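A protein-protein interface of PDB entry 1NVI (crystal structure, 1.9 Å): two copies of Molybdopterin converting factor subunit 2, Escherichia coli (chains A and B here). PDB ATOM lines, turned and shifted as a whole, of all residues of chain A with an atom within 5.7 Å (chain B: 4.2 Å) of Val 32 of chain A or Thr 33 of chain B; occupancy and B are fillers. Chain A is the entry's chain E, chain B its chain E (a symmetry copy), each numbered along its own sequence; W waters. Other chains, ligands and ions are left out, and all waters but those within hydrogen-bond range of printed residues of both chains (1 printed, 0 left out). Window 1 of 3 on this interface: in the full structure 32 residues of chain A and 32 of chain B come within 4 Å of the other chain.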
ATOM      1  N   TYR A  19      -7.801   1.611  20.004  1.00  0.00           N
ATOM      2  CA  TYR A  19      -6.947   1.159  21.092  1.00  0.00           C
ATOM      3  C   TYR A  19      -6.787   2.187  22.217  1.00  0.00           C
ATOM      4  O   TYR A  19      -6.909   1.826  23.383  1.00  0.00           O
ATOM      5  CB  TYR A  19      -5.565   0.694  20.590  1.00  0.00           C
ATOM      6  CG  TYR A  19      -4.644   0.321  21.726  1.00  0.00           C
ATOM      7  CD1 TYR A  19      -4.672  -0.962  22.276  1.00  0.00           C
ATOM      8  CD2 TYR A  19      -3.785   1.258  22.279  1.00  0.00           C
ATOM      9  CE1 TYR A  19      -3.860  -1.297  23.328  1.00  0.00           C
ATOM     10  CE2 TYR A  19      -2.969   0.939  23.332  1.00  0.00           C
ATOM     11  CZ  TYR A  19      -3.010  -0.347  23.848  1.00  0.00           C
ATOM     12  OH  TYR A  19      -2.202  -0.669  24.888  1.00  0.00           O
ATOM     13  N   LEU A  22      -9.590   2.167  24.814  1.00  0.00           N
ATOM     14  CA  LEU A  22      -9.530   0.917  25.556  1.00  0.00           C
ATOM     15  C   LEU A  22      -8.441   0.947  26.625  1.00  0.00           C
ATOM     16  O   LEU A  22      -8.664   0.535  27.761  1.00  0.00           O
ATOM     17  CB  LEU A  22      -9.273  -0.203  24.551  1.00  0.00           C
ATOM     18  CG  LEU A  22      -9.812  -1.591  24.747  1.00  0.00           C
ATOM     19  CD1 LEU A  22     -11.307  -1.614  24.976  1.00  0.00           C
ATOM     20  CD2 LEU A  22      -9.369  -2.394  23.490  1.00  0.00           C
ATOM     21  N   ALA A  30      -3.943  -5.044  31.640  1.00  0.00           N
ATOM     22  CA  ALA A  30      -3.895  -5.930  30.465  1.00  0.00           C
ATOM     23  C   ALA A  30      -4.897  -5.488  29.413  1.00  0.00           C
ATOM     24  O   ALA A  30      -6.051  -5.244  29.743  1.00  0.00           O
ATOM     25  CB  ALA A  30      -4.186  -7.372  30.876  1.00  0.00           C
ATOM     26  N   VAL A  31      -4.458  -5.416  28.161  1.00  0.00           N
ATOM     27  CA  VAL A  31      -5.324  -5.091  27.026  1.00  0.00           C
ATOM     28  C   VAL A  31      -5.140  -6.140  25.917  1.00  0.00           C
ATOM     29  O   VAL A  31      -4.043  -6.305  25.381  1.00  0.00           O
ATOM     30  CB  VAL A  31      -5.024  -3.684  26.450  1.00  0.00           C
ATOM     31  CG1 VAL A  31      -5.977  -3.372  25.274  1.00  0.00           C
ATOM     32  CG2 VAL A  31      -5.098  -2.603  27.559  1.00  0.00           C
ATOM     33  N   VAL A  32      -6.226  -6.829  25.574  1.00  0.00           N
ATOM     34  CA  VAL A  32      -6.239  -7.800  24.502  1.00  0.00           C
ATOM     35  C   VAL A  32      -7.121  -7.322  23.348  1.00  0.00           C
ATOM     36  O   VAL A  32      -8.240  -6.916  23.571  1.00  0.00           O
ATOM     37  CB  VAL A  32      -6.722  -9.163  25.003  1.00  0.00           C
ATOM     38  CG1 VAL A  32      -7.032 -10.101  23.836  1.00  0.00           C
ATOM     39  CG2 VAL A  32      -5.656  -9.789  25.906  1.00  0.00           C
ATOM     40  N   THR A  33      -6.617  -7.369  22.113  1.00  0.00           N
ATOM     41  CA  THR A  33      -7.467  -7.127  20.951  1.00  0.00           C
ATOM     42  C   THR A  33      -7.474  -8.316  20.006  1.00  0.00           C
ATOM     43  O   THR A  33      -6.484  -9.052  19.897  1.00  0.00           O
ATOM     44  CB  THR A  33      -7.062  -5.839  20.176  1.00  0.00           C
ATOM     45  OG1 THR A  33      -5.838  -6.031  19.452  1.00  0.00           O
ATOM     46  CG2 THR A  33      -6.804  -4.656  21.123  1.00  0.00           C
ATOM     47  N   PHE A  34      -8.599  -8.475  19.310  1.00  0.00           N
ATOM     48  CA  PHE A  34      -8.719  -9.398  18.211  1.00  0.00           C
ATOM     49  C   PHE A  34      -9.300  -8.658  17.004  1.00  0.00           C
ATOM     50  O   PHE A  34     -10.325  -7.978  17.118  1.00  0.00           O
ATOM     51  CB  PHE A  34      -9.623 -10.604  18.542  1.00  0.00           C
ATOM     52  CG  PHE A  34      -9.883 -11.493  17.338  1.00  0.00           C
ATOM     53  CD1 PHE A  34      -9.005 -12.496  17.002  1.00  0.00           C
ATOM     54  CD2 PHE A  34     -10.996 -11.278  16.523  1.00  0.00           C
ATOM     55  CE1 PHE A  34      -9.225 -13.265  15.857  1.00  0.00           C
ATOM     56  CE2 PHE A  34     -11.228 -12.047  15.412  1.00  0.00           C
ATOM     57  CZ  PHE A  34     -10.348 -13.027  15.068  1.00  0.00           C
ATOM     58  N   VAL A  97     -12.654  -6.951  18.566  1.00  0.00           N
ATOM     59  CA  VAL A  97     -12.998  -7.128  19.971  1.00  0.00           C
ATOM     60  C   VAL A  97     -11.812  -6.676  20.809  1.00  0.00           C
ATOM     61  O   VAL A  97     -10.703  -7.158  20.628  1.00  0.00           O
ATOM     62  CB  VAL A  97     -13.339  -8.605  20.264  1.00  0.00           C
ATOM     63  CG1 VAL A  97     -13.506  -8.845  21.764  1.00  0.00           C
ATOM     64  CG2 VAL A  97     -14.605  -9.009  19.505  1.00  0.00           C
ATOM     65  N   GLY A  98     -12.053  -5.751  21.728  1.00  0.00           N
ATOM     66  CA  GLY A  98     -11.047  -5.298  22.671  1.00  0.00           C
ATOM     67  C   GLY A  98     -11.553  -5.440  24.091  1.00  0.00           C
ATOM     68  O   GLY A  98     -12.689  -5.061  24.393  1.00  0.00           O
ATOM     69  N   VAL A  99     -10.717  -6.003  24.962  1.00  0.00           N
ATOM     70  CA  VAL A  99     -11.077  -6.254  26.369  1.00  0.00           C
ATOM     71  C   VAL A  99      -9.908  -5.831  27.260  1.00  0.00           C
ATOM     72  O   VAL A  99      -8.750  -6.005  26.901  1.00  0.00           O
ATOM     73  CB  VAL A  99     -11.367  -7.767  26.598  1.00  0.00           C
ATOM     74  CG1 VAL A  99     -11.598  -8.072  28.066  1.00  0.00           C
ATOM     75  CG2 VAL A  99     -12.561  -8.220  25.764  1.00  0.00           C
ATOM     76  N   THR A 100     -10.213  -5.270  28.418  1.00  0.00           N
ATOM     77  CA  THR A 100      -9.196  -4.952  29.403  1.00  0.00           C
ATOM     78  C   THR A 100      -9.537  -5.640  30.731  1.00  0.00           C
ATOM     79  O   THR A 100     -10.701  -5.954  31.026  1.00  0.00           O
ATOM     80  CB  THR A 100      -9.110  -3.438  29.631  1.00  0.00           C
ATOM     81  OG1 THR A 100     -10.304  -2.980  30.267  1.00  0.00           O
ATOM     82  CG2 THR A 100      -9.060  -2.654  28.336  1.00  0.00           C
ATOM     83  N   ARG A 104      -3.735 -10.625  32.787  1.00  0.00           N
ATOM     84  CA  ARG A 104      -3.771 -11.054  31.389  1.00  0.00           C
ATOM     85  C   ARG A 104      -4.719 -12.226  31.119  1.00  0.00           C
ATOM     86  O   ARG A 104      -5.342 -12.265  30.062  1.00  0.00           O
ATOM     87  CB  ARG A 104      -2.365 -11.379  30.859  1.00  0.00           C
ATOM     88  CG  ARG A 104      -1.706 -12.624  31.410  1.00  0.00           C
ATOM     89  CD  ARG A 104      -0.240 -12.720  31.047  1.00  0.00           C
ATOM     90  NE  ARG A 104       0.329 -14.009  31.404  1.00  0.00           N
ATOM     91  CZ  ARG A 104       0.728 -14.365  32.613  1.00  0.00           C
ATOM     92  NH1 ARG A 104       0.638 -13.518  33.642  1.00  0.00           N
ATOM     93  NH2 ARG A 104       1.220 -15.584  32.803  1.00  0.00           N
ATOM     94  N   ALA A 107      -8.314 -11.129  30.342  1.00  0.00           N
ATOM     95  CA  ALA A 107      -8.440 -10.430  29.068  1.00  0.00           C
ATOM     96  C   ALA A 107      -8.384 -11.409  27.866  1.00  0.00           C
ATOM     97  O   ALA A 107      -9.187 -11.304  26.940  1.00  0.00           O
ATOM     98  CB  ALA A 107      -7.390  -9.347  28.955  1.00  0.00           C
ATOM     99  N   PHE A 108      -7.474 -12.377  27.913  1.00  0.00           N
ATOM    100  CA  PHE A 108      -7.335 -13.362  26.836  1.00  0.00           C
ATOM    101  C   PHE A 108      -8.575 -14.254  26.752  1.00  0.00           C
ATOM    102  O   PHE A 108      -9.073 -14.568  25.653  1.00  0.00           O
ATOM    103  CB  PHE A 108      -6.112 -14.254  27.057  1.00  0.00           C
ATOM    104  CG  PHE A 108      -4.820 -13.711  26.478  1.00  0.00           C
ATOM    105  CD1 PHE A 108      -3.761 -13.383  27.307  1.00  0.00           C
ATOM    106  CD2 PHE A 108      -4.665 -13.536  25.113  1.00  0.00           C
ATOM    107  CE1 PHE A 108      -2.573 -12.885  26.787  1.00  0.00           C
ATOM    108  CE2 PHE A 108      -3.484 -13.069  24.586  1.00  0.00           C
ATOM    109  CZ  PHE A 108      -2.433 -12.739  25.414  1.00  0.00           C
ATOM    110  N   GLY A 111     -11.735 -12.227  25.715  1.00  0.00           N
ATOM    111  CA  GLY A 111     -11.649 -11.857  24.315  1.00  0.00           C
ATOM    112  C   GLY A 111     -12.055 -13.019  23.405  1.00  0.00           C
ATOM    113  O   GLY A 111     -12.780 -12.826  22.415  1.00  0.00           O
ATOM    114  N   LEU B  22       1.717  -5.816  11.361  1.00  0.00           N
ATOM    115  CA  LEU B  22       1.191  -7.118  11.742  1.00  0.00           C
ATOM    116  C   LEU B  22       0.030  -7.542  10.847  1.00  0.00           C
ATOM    117  O   LEU B  22      -0.030  -8.683  10.393  1.00  0.00           O
ATOM    118  CB  LEU B  22       0.747  -7.026  13.199  1.00  0.00           C
ATOM    119  CG  LEU B  22       0.818  -8.201  14.132  1.00  0.00           C
ATOM    120  CD1 LEU B  22       2.195  -8.825  14.187  1.00  0.00           C
ATOM    121  CD2 LEU B  22       0.325  -7.674  15.510  1.00  0.00           C
ATOM    122  N   VAL B  32      -4.239 -11.029  16.854  1.00  0.00           N
ATOM    123  CA  VAL B  32      -4.375 -10.876  18.286  1.00  0.00           C
ATOM    124  C   VAL B  32      -3.248 -10.009  18.848  1.00  0.00           C
ATOM    125  O   VAL B  32      -2.098 -10.245  18.550  1.00  0.00           O
ATOM    126  CB  VAL B  32      -4.389 -12.238  18.984  1.00  0.00           C
ATOM    127  CG1 VAL B  32      -4.223 -12.083  20.495  1.00  0.00           C
ATOM    128  CG2 VAL B  32      -5.701 -12.962  18.675  1.00  0.00           C
ATOM    129  N   THR B  33      -3.577  -9.003  19.661  1.00  0.00           N
ATOM    130  CA  THR B  33      -2.549  -8.270  20.394  1.00  0.00           C
ATOM    131  C   THR B  33      -2.772  -8.343  21.894  1.00  0.00           C
ATOM    132  O   THR B  33      -3.913  -8.434  22.367  1.00  0.00           O
ATOM    133  CB  THR B  33      -2.447  -6.781  19.947  1.00  0.00           C
ATOM    134  OG1 THR B  33      -3.568  -6.020  20.420  1.00  0.00           O
ATOM    135  CG2 THR B  33      -2.464  -6.639  18.416  1.00  0.00           C
ATOM    136  N   PHE B  34      -1.664  -8.278  22.632  1.00  0.00           N
ATOM    137  CA  PHE B  34      -1.682  -8.107  24.062  1.00  0.00           C
ATOM    138  C   PHE B  34      -0.754  -6.948  24.433  1.00  0.00           C
ATOM    139  O   PHE B  34       0.403  -6.906  24.002  1.00  0.00           O
ATOM    140  CB  PHE B  34      -1.229  -9.373  24.819  1.00  0.00           C
ATOM    141  CG  PHE B  34      -1.090  -9.147  26.314  1.00  0.00           C
ATOM    142  CD1 PHE B  34      -2.174  -9.276  27.149  1.00  0.00           C
ATOM    143  CD2 PHE B  34       0.133  -8.757  26.864  1.00  0.00           C
ATOM    144  CE1 PHE B  34      -2.045  -9.005  28.513  1.00  0.00           C
ATOM    145  CE2 PHE B  34       0.270  -8.514  28.205  1.00  0.00           C
ATOM    146  CZ  PHE B  34      -0.809  -8.623  29.028  1.00  0.00           C
ATOM    147  N   PHE B  96       4.391  -5.678  24.557  1.00  0.00           N
ATOM    148  CA  PHE B  96       3.451  -5.849  23.458  1.00  0.00           C
ATOM    149  C   PHE B  96       3.752  -7.175  22.771  1.00  0.00           C
ATOM    150  O   PHE B  96       4.907  -7.464  22.465  1.00  0.00           O
ATOM    151  CB  PHE B  96       3.594  -4.705  22.455  1.00  0.00           C
ATOM    152  CG  PHE B  96       2.748  -4.867  21.211  1.00  0.00           C
ATOM    153  CD1 PHE B  96       1.401  -4.514  21.220  1.00  0.00           C
ATOM    154  CD2 PHE B  96       3.298  -5.369  20.033  1.00  0.00           C
ATOM    155  CE1 PHE B  96       0.605  -4.649  20.051  1.00  0.00           C
ATOM    156  CE2 PHE B  96       2.514  -5.512  18.882  1.00  0.00           C
ATOM    157  CZ  PHE B  96       1.152  -5.155  18.907  1.00  0.00           C
ATOM    158  N   VAL B  97       2.721  -7.989  22.578  1.00  0.00           N
ATOM    159  CA  VAL B  97       2.810  -9.211  21.789  1.00  0.00           C
ATOM    160  C   VAL B  97       1.713  -9.175  20.736  1.00  0.00           C
ATOM    161  O   VAL B  97       0.545  -9.019  21.061  1.00  0.00           O
ATOM    162  CB  VAL B  97       2.655 -10.454  22.692  1.00  0.00           C
ATOM    163  CG1 VAL B  97       2.545 -11.730  21.860  1.00  0.00           C
ATOM    164  CG2 VAL B  97       3.831 -10.540  23.668  1.00  0.00           C
HETATM  165  O   HOH W   1      -3.289  -4.927  23.010  1.00  0.00           O
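OG1 of Thr 33 of chain B is in hydrogen-bond range of OG1 of Thr 33 of chain A, at 2.5 Å.
N of Phe 34 of chain B lies within hydrogen-bond range of O of Val 97 of chain B. N of Val 32 of chain A is in hydrogen-bond range of O of Val 99 of chain A, at 3.0 Å. The backbone carbonyl oxygen (O) of Val 97 of chain A lies within hydrogen-bond range of the backbone NH (N) of Phe 34 of chain A, 2.8 Å away.
Among the printed residues, merely in contact across the chains: Thr 33 of chain A with Val 32 of chain B (3.2 Å), Val 32 of chain A with Thr 33 of chain B (3.2 Å), Val 31 of chain A with Phe 34 of chain B (3.2 Å), Arg 104 of chain A with Phe 34 of chain B (3.4 Å), Ala 30 of chain A with Phe 34 of chain B (3.6 Å), Phe 108 of chain A with Phe 34 of chain B (3.6 Å), Val 31 of chain A with Thr 33 of chain B (3.7 Å), Phe 34 of chain A with Val 32 of chain B (3.7 Å) and Val 32 of chain A with Phe 34 of chain B (3.7 Å).
Tyr 19 of chain A touches none of the printed residues of chain B. Of the printed residues of chain B, Ala 30 of chain A touches Phe 34 (3.6 Å). Printed residues of chain B within 4 Å of Val 31 of chain A: Thr 33 and Phe 34. Printed residues of chain B within 4 Å of Thr 33 of chain A: Val 32 (3.2 Å) and Thr 33 (2.5 Å). Gly 98 of chain A touches none of the printed residues of chain B. Of the printed residues of chain A, Val 32 of chain B touches Thr 33 and Phe 34. Thr 33 of chain B touches just these residues of chain A: Val 31 (3.7 Å), Val 32 (3.2 Å) and Thr 33 (2.5 Å). Of the printed residues of chain A, Phe 34 of chain B touches Ala 30, Val 31, Val 32, Arg 104 and Phe 108. The nearest printed residue of chain B that does not touch Phe 108 of chain A is Val 32 of chain B (4.3 Å).
Of the 6 printed residues of chain B, 3 touch a printed residue of chain A. Printed residues of chain A that touch a printed residue of chain B: Ala 30, Val 31, Val 32, Thr 33, Phe 34, Arg 104 and Phe 108. Hydrophobic or aromatic side chains of chain A within 4 Å of the printed part of chain B: Ala 30, Val 32, Phe 34 and Phe 108. Among the printed residues, 10 pairs touch across the chains. Among the printed residues, no Asp or Glu carboxylate lies within 4 Å of a Lys or Arg side-chain nitrogen of the other chain.
Val 32 of chain A touches Thr 33 of chain B, and with the chains exchanged Thr 33 of chain A touches Val 32 of chain B. Val 32 of chain A touches Phe 34 of chain B, and with the chains exchanged Phe 34 of chain A touches Val 32 of chain B. Thr 33 of chain B touches its own counterpart, Thr 33 of chain A. Positions printed for both chains: 22, 32, 33, 34 and 97.
Water W1 lies within hydrogen-bond range of the side-chain hydroxyl of Thr 33 of chain B (2.8 Å) and the backbone carbonyl oxygen of Val 31 of chain A (2.8 Å).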
